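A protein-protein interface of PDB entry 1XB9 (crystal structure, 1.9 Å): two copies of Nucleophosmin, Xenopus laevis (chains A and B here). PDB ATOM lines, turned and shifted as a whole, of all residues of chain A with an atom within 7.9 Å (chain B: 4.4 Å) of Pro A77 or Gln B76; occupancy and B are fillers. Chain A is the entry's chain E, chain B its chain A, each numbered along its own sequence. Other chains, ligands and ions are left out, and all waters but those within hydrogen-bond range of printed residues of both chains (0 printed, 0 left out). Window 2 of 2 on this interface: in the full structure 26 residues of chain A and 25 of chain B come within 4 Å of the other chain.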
ATOM      1  N   THR A  38      -6.163  18.193  29.206  1.00  0.00           N
ATOM      2  CA  THR A  38      -7.439  18.140  28.535  1.00  0.00           C
ATOM      3  C   THR A  38      -8.600  18.027  29.470  1.00  0.00           C
ATOM      4  O   THR A  38      -8.462  17.486  30.537  1.00  0.00           O
ATOM      5  CB  THR A  38      -7.588  17.019  27.462  1.00  0.00           C
ATOM      6  OG1 THR A  38      -7.454  15.767  28.118  1.00  0.00           O
ATOM      7  CG2 THR A  38      -6.506  17.082  26.367  1.00  0.00           C
ATOM      8  N   VAL A  39      -9.747  18.507  29.059  1.00  0.00           N
ATOM      9  CA  VAL A  39     -11.015  18.242  29.681  1.00  0.00           C
ATOM     10  C   VAL A  39     -11.897  17.512  28.664  1.00  0.00           C
ATOM     11  O   VAL A  39     -11.994  17.970  27.537  1.00  0.00           O
ATOM     12  CB  VAL A  39     -11.675  19.547  30.132  1.00  0.00           C
ATOM     13  CG1 VAL A  39     -12.843  19.214  30.943  1.00  0.00           C
ATOM     14  CG2 VAL A  39     -10.645  20.375  30.886  1.00  0.00           C
ATOM     15  N   SER A  40     -12.551  16.408  29.023  1.00  0.00           N
ATOM     16  CA  SER A  40     -13.263  15.622  28.014  1.00  0.00           C
ATOM     17  C   SER A  40     -14.484  14.951  28.634  1.00  0.00           C
ATOM     18  O   SER A  40     -14.459  14.620  29.828  1.00  0.00           O
ATOM     19  CB  SER A  40     -12.391  14.505  27.425  1.00  0.00           C
ATOM     20  OG  SER A  40     -12.016  13.676  28.450  1.00  0.00           O
ATOM     21  N   LEU A  41     -15.532  14.836  27.831  1.00  0.00           N
ATOM     22  CA  LEU A  41     -16.763  14.207  28.281  1.00  0.00           C
ATOM     23  C   LEU A  41     -16.769  12.713  28.053  1.00  0.00           C
ATOM     24  O   LEU A  41     -16.304  12.170  27.014  1.00  0.00           O
ATOM     25  CB  LEU A  41     -17.900  14.870  27.615  1.00  0.00           C
ATOM     26  CG  LEU A  41     -18.037  16.324  27.875  1.00  0.00           C
ATOM     27  CD1 LEU A  41     -19.171  16.943  27.085  1.00  0.00           C
ATOM     28  CD2 LEU A  41     -18.161  16.572  29.349  1.00  0.00           C
ATOM     29  N   GLY A  42     -17.228  11.984  29.058  1.00  0.00           N
ATOM     30  CA  GLY A  42     -17.380  10.531  28.945  1.00  0.00           C
ATOM     31  C   GLY A  42     -18.506  10.155  27.978  1.00  0.00           C
ATOM     32  O   GLY A  42     -19.330  10.967  27.567  1.00  0.00           O
ATOM     33  N   SER A  70     -16.247  24.893  29.104  1.00  0.00           N
ATOM     34  CA  SER A  70     -17.626  24.509  28.786  1.00  0.00           C
ATOM     35  C   SER A  70     -17.643  23.598  27.565  1.00  0.00           C
ATOM     36  O   SER A  70     -17.046  23.942  26.518  1.00  0.00           O
ATOM     37  CB  SER A  70     -18.466  25.715  28.358  1.00  0.00           C
ATOM     38  OG  SER A  70     -18.464  26.669  29.333  1.00  0.00           O
ATOM     39  N   LEU A  71     -18.258  22.424  27.721  1.00  0.00           N
ATOM     40  CA  LEU A  71     -18.205  21.375  26.724  1.00  0.00           C
ATOM     41  C   LEU A  71     -19.575  20.849  26.574  1.00  0.00           C
ATOM     42  O   LEU A  71     -20.421  20.951  27.531  1.00  0.00           O
ATOM     43  CB  LEU A  71     -17.384  20.183  27.254  1.00  0.00           C
ATOM     44  CG  LEU A  71     -16.029  20.368  27.903  1.00  0.00           C
ATOM     45  CD1 LEU A  71     -16.255  20.713  29.447  1.00  0.00           C
ATOM     46  CD2 LEU A  71     -15.325  18.993  27.815  1.00  0.00           C
ATOM     47  N   LYS A  72     -19.829  20.211  25.440  1.00  0.00           N
ATOM     48  CA  LYS A  72     -21.101  19.602  25.155  1.00  0.00           C
ATOM     49  C   LYS A  72     -20.883  18.503  24.208  1.00  0.00           C
ATOM     50  O   LYS A  72     -20.220  18.735  23.149  1.00  0.00           O
ATOM     51  CB  LYS A  72     -22.043  20.638  24.550  1.00  0.00           C
ATOM     52  CG  LYS A  72     -23.565  20.039  24.415  1.00  0.00           C
ATOM     53  CD  LYS A  72     -24.693  21.124  23.930  1.00  0.00           C
ATOM     54  CE  LYS A  72     -25.969  20.366  23.394  1.00  0.00           C
ATOM     55  NZ  LYS A  72     -26.941  21.397  23.250  1.00  0.00           N
ATOM     56  N   PRO A  73     -21.465  17.339  24.437  1.00  0.00           N
ATOM     57  CA  PRO A  73     -21.105  16.175  23.618  1.00  0.00           C
ATOM     58  C   PRO A  73     -21.366  16.300  22.113  1.00  0.00           C
ATOM     59  O   PRO A  73     -20.529  15.789  21.435  1.00  0.00           O
ATOM     60  CB  PRO A  73     -21.836  14.998  24.247  1.00  0.00           C
ATOM     61  CG  PRO A  73     -22.288  15.477  25.503  1.00  0.00           C
ATOM     62  CD  PRO A  73     -22.395  16.950  25.513  1.00  0.00           C
ATOM     63  N   SER A  74     -22.443  16.961  21.624  1.00  0.00           N
ATOM     64  CA  SER A  74     -22.678  17.025  20.221  1.00  0.00           C
ATOM     65  C   SER A  74     -21.961  18.263  19.582  1.00  0.00           C
ATOM     66  O   SER A  74     -22.201  18.525  18.381  1.00  0.00           O
ATOM     67  CB  SER A  74     -24.201  17.027  19.943  1.00  0.00           C
ATOM     68  OG  SER A  74     -24.780  18.142  20.617  1.00  0.00           O
ATOM     69  N   VAL A  75     -21.184  19.048  20.367  1.00  0.00           N
ATOM     70  CA  VAL A  75     -20.611  20.301  19.834  1.00  0.00           C
ATOM     71  C   VAL A  75     -19.087  20.347  19.963  1.00  0.00           C
ATOM     72  O   VAL A  75     -18.403  20.660  19.030  1.00  0.00           O
ATOM     73  CB  VAL A  75     -21.198  21.546  20.610  1.00  0.00           C
ATOM     74  CG1 VAL A  75     -20.538  22.833  20.276  1.00  0.00           C
ATOM     75  CG2 VAL A  75     -22.764  21.623  20.444  1.00  0.00           C
ATOM     76  N   GLN A  76     -18.600  20.026  21.173  1.00  0.00           N
ATOM     77  CA  GLN A  76     -17.184  20.085  21.524  1.00  0.00           C
ATOM     78  C   GLN A  76     -16.991  19.169  22.740  1.00  0.00           C
ATOM     79  O   GLN A  76     -17.016  19.649  23.857  1.00  0.00           O
ATOM     80  CB  GLN A  76     -16.837  21.557  21.839  1.00  0.00           C
ATOM     81  CG  GLN A  76     -15.439  21.802  22.214  1.00  0.00           C
ATOM     82  CD  GLN A  76     -15.110  23.248  22.425  1.00  0.00           C
ATOM     83  OE1 GLN A  76     -15.968  24.152  22.626  1.00  0.00           O
ATOM     84  NE2 GLN A  76     -13.830  23.497  22.394  1.00  0.00           N
ATOM     85  N   PRO A  77     -16.867  17.851  22.518  1.00  0.00           N
ATOM     86  CA  PRO A  77     -16.667  16.934  23.634  1.00  0.00           C
ATOM     87  C   PRO A  77     -15.263  16.955  24.293  1.00  0.00           C
ATOM     88  O   PRO A  77     -15.161  16.519  25.478  1.00  0.00           O
ATOM     89  CB  PRO A  77     -16.935  15.555  23.007  1.00  0.00           C
ATOM     90  CG  PRO A  77     -16.591  15.765  21.489  1.00  0.00           C
ATOM     91  CD  PRO A  77     -16.959  17.118  21.248  1.00  0.00           C
ATOM     92  N   THR A  78     -14.263  17.572  23.645  1.00  0.00           N
ATOM     93  CA  THR A  78     -12.953  17.788  24.260  1.00  0.00           C
ATOM     94  C   THR A  78     -12.391  19.178  24.060  1.00  0.00           C
ATOM     95  O   THR A  78     -12.496  19.819  23.007  1.00  0.00           O
ATOM     96  CB  THR A  78     -11.900  16.715  23.698  1.00  0.00           C
ATOM     97  OG1 THR A  78     -12.423  15.439  23.987  1.00  0.00           O
ATOM     98  CG2 THR A  78     -10.533  16.739  24.384  1.00  0.00           C
ATOM     99  N   VAL A  79     -11.809  19.629  25.147  1.00  0.00           N
ATOM    100  CA  VAL A  79     -11.142  20.869  25.282  1.00  0.00           C
ATOM    101  C   VAL A  79      -9.684  20.614  25.722  1.00  0.00           C
ATOM    102  O   VAL A  79      -9.405  19.997  26.776  1.00  0.00           O
ATOM    103  CB  VAL A  79     -11.900  21.798  26.264  1.00  0.00           C
ATOM    104  CG1 VAL A  79     -11.152  22.932  26.554  1.00  0.00           C
ATOM    105  CG2 VAL A  79     -13.305  22.270  25.785  1.00  0.00           C
ATOM    106  N   SER A  80      -8.740  21.110  24.953  1.00  0.00           N
ATOM    107  CA  SER A  80      -7.341  20.945  25.254  1.00  0.00           C
ATOM    108  C   SER A  80      -6.887  22.252  25.830  1.00  0.00           C
ATOM    109  O   SER A  80      -7.057  23.245  25.211  1.00  0.00           O
ATOM    110  CB  SER A  80      -6.538  20.569  24.013  1.00  0.00           C
ATOM    111  OG  SER A  80      -5.142  20.609  24.321  1.00  0.00           O
ATOM    112  N   PRO A 100     -20.282  11.921  33.128  1.00  0.00           N
ATOM    113  CA  PRO A 100     -18.963  12.235  33.702  1.00  0.00           C
ATOM    114  C   PRO A 100     -18.058  13.087  32.783  1.00  0.00           C
ATOM    115  O   PRO A 100     -18.146  12.953  31.540  1.00  0.00           O
ATOM    116  CB  PRO A 100     -18.323  10.907  33.867  1.00  0.00           C
ATOM    117  CG  PRO A 100     -18.969   9.974  33.014  1.00  0.00           C
ATOM    118  CD  PRO A 100     -20.317  10.571  32.545  1.00  0.00           C
ATOM    119  N   VAL A 101     -17.174  13.794  33.422  1.00  0.00           N
ATOM    120  CA  VAL A 101     -16.200  14.704  32.787  1.00  0.00           C
ATOM    121  C   VAL A 101     -14.817  14.296  33.318  1.00  0.00           C
ATOM    122  O   VAL A 101     -14.664  14.001  34.555  1.00  0.00           O
ATOM    123  CB  VAL A 101     -16.449  16.206  33.110  1.00  0.00           C
ATOM    124  CG1 VAL A 101     -15.552  16.989  32.240  1.00  0.00           C
ATOM    125  CG2 VAL A 101     -17.844  16.609  32.724  1.00  0.00           C
ATOM    126  N   TYR A 102     -13.810  14.302  32.460  1.00  0.00           N
ATOM    127  CA  TYR A 102     -12.443  13.868  32.883  1.00  0.00           C
ATOM    128  C   TYR A 102     -11.526  15.021  32.718  1.00  0.00           C
ATOM    129  O   TYR A 102     -11.686  15.845  31.824  1.00  0.00           O
ATOM    130  CB  TYR A 102     -11.963  12.686  32.079  1.00  0.00           C
ATOM    131  CG  TYR A 102     -12.834  11.476  32.323  1.00  0.00           C
ATOM    132  CD1 TYR A 102     -14.050  11.311  31.593  1.00  0.00           C
ATOM    133  CD2 TYR A 102     -12.527  10.552  33.265  1.00  0.00           C
ATOM    134  CE1 TYR A 102     -14.933  10.192  31.826  1.00  0.00           C
ATOM    135  CE2 TYR A 102     -13.418   9.397  33.515  1.00  0.00           C
ATOM    136  CZ  TYR A 102     -14.581   9.264  32.843  1.00  0.00           C
ATOM    137  OH  TYR A 102     -15.380   8.229  33.125  1.00  0.00           O
ATOM    138  N   LEU B  49     -19.207   8.597  20.092  1.00  0.00           N
ATOM    139  CA  LEU B  49     -18.072   8.980  20.962  1.00  0.00           C
ATOM    140  C   LEU B  49     -17.040   7.866  21.121  1.00  0.00           C
ATOM    141  O   LEU B  49     -17.328   6.693  21.292  1.00  0.00           O
ATOM    142  CB  LEU B  49     -18.548   9.547  22.331  1.00  0.00           C
ATOM    143  CG  LEU B  49     -17.613  10.665  22.829  1.00  0.00           C
ATOM    144  CD1 LEU B  49     -17.735  11.880  21.863  1.00  0.00           C
ATOM    145  CD2 LEU B  49     -18.075  11.188  24.201  1.00  0.00           C
ATOM    146  N   SER B  70     -11.912  12.652  23.934  1.00  0.00           N
ATOM    147  CA  SER B  70     -13.177  12.149  23.465  1.00  0.00           C
ATOM    148  C   SER B  70     -13.448  12.773  22.064  1.00  0.00           C
ATOM    149  O   SER B  70     -13.441  13.973  21.943  1.00  0.00           O
ATOM    150  CB  SER B  70     -14.331  12.622  24.394  1.00  0.00           C
ATOM    151  OG  SER B  70     -14.203  11.938  25.567  1.00  0.00           O
ATOM    152  N   LEU B  71     -13.696  11.952  21.058  1.00  0.00           N
ATOM    153  CA  LEU B  71     -13.861  12.400  19.690  1.00  0.00           C
ATOM    154  C   LEU B  71     -15.055  11.697  19.030  1.00  0.00           C
ATOM    155  O   LEU B  71     -15.317  10.573  19.357  1.00  0.00           O
ATOM    156  CB  LEU B  71     -12.584  11.911  18.907  1.00  0.00           C
ATOM    157  CG  LEU B  71     -11.200  12.149  19.449  1.00  0.00           C
ATOM    158  CD1 LEU B  71     -10.778  11.050  20.491  1.00  0.00           C
ATOM    159  CD2 LEU B  71     -10.173  12.111  18.320  1.00  0.00           C
ATOM    160  N   LYS B  72     -15.586  12.312  17.986  1.00  0.00           N
ATOM    161  CA  LYS B  72     -16.656  11.778  17.223  1.00  0.00           C
ATOM    162  C   LYS B  72     -16.571  12.341  15.839  1.00  0.00           C
ATOM    163  O   LYS B  72     -16.467  13.566  15.682  1.00  0.00           O
ATOM    164  CB  LYS B  72     -18.040  12.157  17.838  1.00  0.00           C
ATOM    165  CG  LYS B  72     -19.276  11.700  17.013  1.00  0.00           C
ATOM    166  CD  LYS B  72     -20.604  11.875  17.898  1.00  0.00           C
ATOM    167  CE  LYS B  72     -21.843  11.254  17.216  1.00  0.00           C
ATOM    168  NZ  LYS B  72     -23.117  11.414  18.018  1.00  0.00           N
ATOM    169  N   SER B  74     -18.554  13.171  13.440  1.00  0.00           N
ATOM    170  CA  SER B  74     -19.346  14.288  12.889  1.00  0.00           C
ATOM    171  C   SER B  74     -19.258  15.568  13.750  1.00  0.00           C
ATOM    172  O   SER B  74     -19.898  16.550  13.442  1.00  0.00           O
ATOM    173  CB  SER B  74     -20.827  13.829  12.693  1.00  0.00           C
ATOM    174  OG  SER B  74     -21.282  13.540  13.970  1.00  0.00           O
ATOM    175  N   VAL B  75     -18.509  15.531  14.849  1.00  0.00           N
ATOM    176  CA  VAL B  75     -18.483  16.616  15.775  1.00  0.00           C
ATOM    177  C   VAL B  75     -17.035  17.110  15.865  1.00  0.00           C
ATOM    178  O   VAL B  75     -16.758  18.257  15.668  1.00  0.00           O
ATOM    179  CB  VAL B  75     -18.931  16.173  17.114  1.00  0.00           C
ATOM    180  CG1 VAL B  75     -18.834  17.280  18.134  1.00  0.00           C
ATOM    181  CG2 VAL B  75     -20.292  15.609  17.021  1.00  0.00           C
ATOM    182  N   GLN B  76     -16.133  16.244  16.159  1.00  0.00           N
ATOM    183  CA  GLN B  76     -14.731  16.594  16.405  1.00  0.00           C
ATOM    184  C   GLN B  76     -13.818  15.383  16.097  1.00  0.00           C
ATOM    185  O   GLN B  76     -13.497  14.631  17.015  1.00  0.00           O
ATOM    186  CB  GLN B  76     -14.574  16.837  17.970  1.00  0.00           C
ATOM    187  CG  GLN B  76     -13.215  17.455  18.322  1.00  0.00           C
ATOM    188  CD  GLN B  76     -13.127  17.945  19.755  1.00  0.00           C
ATOM    189  OE1 GLN B  76     -14.037  17.755  20.563  1.00  0.00           O
ATOM    190  NE2 GLN B  76     -12.044  18.644  20.038  1.00  0.00           N
ATOM    191  N   PRO B  77     -13.436  15.138  14.835  1.00  0.00           N
ATOM    192  CA  PRO B  77     -12.689  13.933  14.511  1.00  0.00           C
ATOM    193  C   PRO B  77     -11.177  13.960  14.911  1.00  0.00           C
ATOM    194  O   PRO B  77     -10.490  12.972  14.829  1.00  0.00           O
ATOM    195  CB  PRO B  77     -12.749  13.884  12.967  1.00  0.00           C
ATOM    196  CG  PRO B  77     -13.090  15.362  12.464  1.00  0.00           C
ATOM    197  CD  PRO B  77     -13.819  15.904  13.672  1.00  0.00           C
ATOM    198  N   THR B  78     -10.635  15.142  15.202  1.00  0.00           N
ATOM    199  CA  THR B  78      -9.220  15.283  15.584  1.00  0.00           C
ATOM    200  C   THR B  78      -9.160  16.190  16.859  1.00  0.00           C
ATOM    201  O   THR B  78      -9.788  17.226  16.878  1.00  0.00           O
ATOM    202  CB  THR B  78      -8.433  16.015  14.520  1.00  0.00           C
ATOM    203  OG1 THR B  78      -8.359  15.221  13.356  1.00  0.00           O
ATOM    204  CG2 THR B  78      -7.008  16.182  15.005  1.00  0.00           C
ATOM    205  N   VAL B  79      -8.278  15.896  17.775  1.00  0.00           N
ATOM    206  CA  VAL B  79      -8.027  16.652  19.020  1.00  0.00           C
ATOM    207  C   VAL B  79      -6.549  16.829  19.137  1.00  0.00           C
ATOM    208  O   VAL B  79      -5.875  15.882  18.956  1.00  0.00           O
ATOM    209  CB  VAL B  79      -8.603  15.813  20.292  1.00  0.00           C
ATOM    210  CG1 VAL B  79      -8.013  16.221  21.615  1.00  0.00           C
ATOM    211  CG2 VAL B  79     -10.088  15.953  20.395  1.00  0.00           C
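The side-chain hydroxyl (OG) of Ser B70 lies within hydrogen-bond range of the backbone carbonyl oxygen (O) of Leu A41 (2.6 Å).
O of Ser B70 is in hydrogen-bond range of OG1 of Thr A78 (2.7 Å).
The side-chain amide oxygen (OE1) of Gln B76 is in hydrogen-bond range of the backbone NH (N) of Thr A78, at 3.1 Å.
N of Pro A77 lies close to OE1 of Gln B76, at 3.4 Å.
The backbone carbonyl oxygen (O) of Ser A40 lies within hydrogen-bond range of the backbone NH (N) of Tyr A102 (2.7 Å).
O of Pro A77 lies within hydrogen-bond range of N of Leu A41 (2.9 Å).
The backbone NH of Gly A42 sits at hydrogen-bond distance from the backbone carbonyl oxygen of Pro A100, 2.8 Å away.
Ser B70 touches Ser A40.
Leu B49 touches Leu A41.
Leu B49 touches Gly A42.
Pro A73 touches Val B75 (O to CG1, 3.999 Å).
C of Ser A74 touches CG1 of Val B75, at 3.6 Å.
Val B75 touches Val A75.
C of Gln A76 touches OE1 of Gln B76, 3.9 Å away.
Pro A77 touches Leu B49.
Pro A77 touches Ser B70.
Val B75 touches Pro A77 (CG1 to CD, 3.6 Å).
Of the printed residues of chain B, Ser A40 touches Ser B70.
Of the printed residues of chain B, Leu A41 touches Leu B49 and Ser B70.
Leu A71 touches none of the printed residues of chain B.
Printed residues of chain B within 4 Å of Val A75: Val B75.
Val A101 touches none of the printed residues of chain B.
Of the printed residues of chain A, Gln B76 touches Gln A76, Pro A77 and Thr A78.
The nearest printed residue of chain B that does not touch Ser A74 is Ser B74 (5.8 Å).
Hydrophobic or aromatic side chains of chain A within 4 Å of the printed part of chain B: Pro A77.
Hydrophobic or aromatic side chains of chain B that line the printed part of chain A: Leu B49, Val B75 and Val B79.
Among the printed residues, no Asp or Glu carboxylate lies within 4 Å of a Lys or Arg side-chain nitrogen of the other chain.
Ser A74 touches Val B75, but with the chains exchanged Val A75 does not touch Ser B74 (7.1 Å).
Val A75 touches its own counterpart, Val B75.
Thr A78 touches Ser B70, but with the chains exchanged Ser A70 does not touch Thr B78 (13.8 Å).
Thr A78 touches Val B79, but with the chains exchanged Val A79 does not touch Thr B78 (8.8 Å).
9 positions are printed for both chains.
Of the 15 pairs that touch across the chains among the printed residues, 2 have their exchanged pair printed and touching as well.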
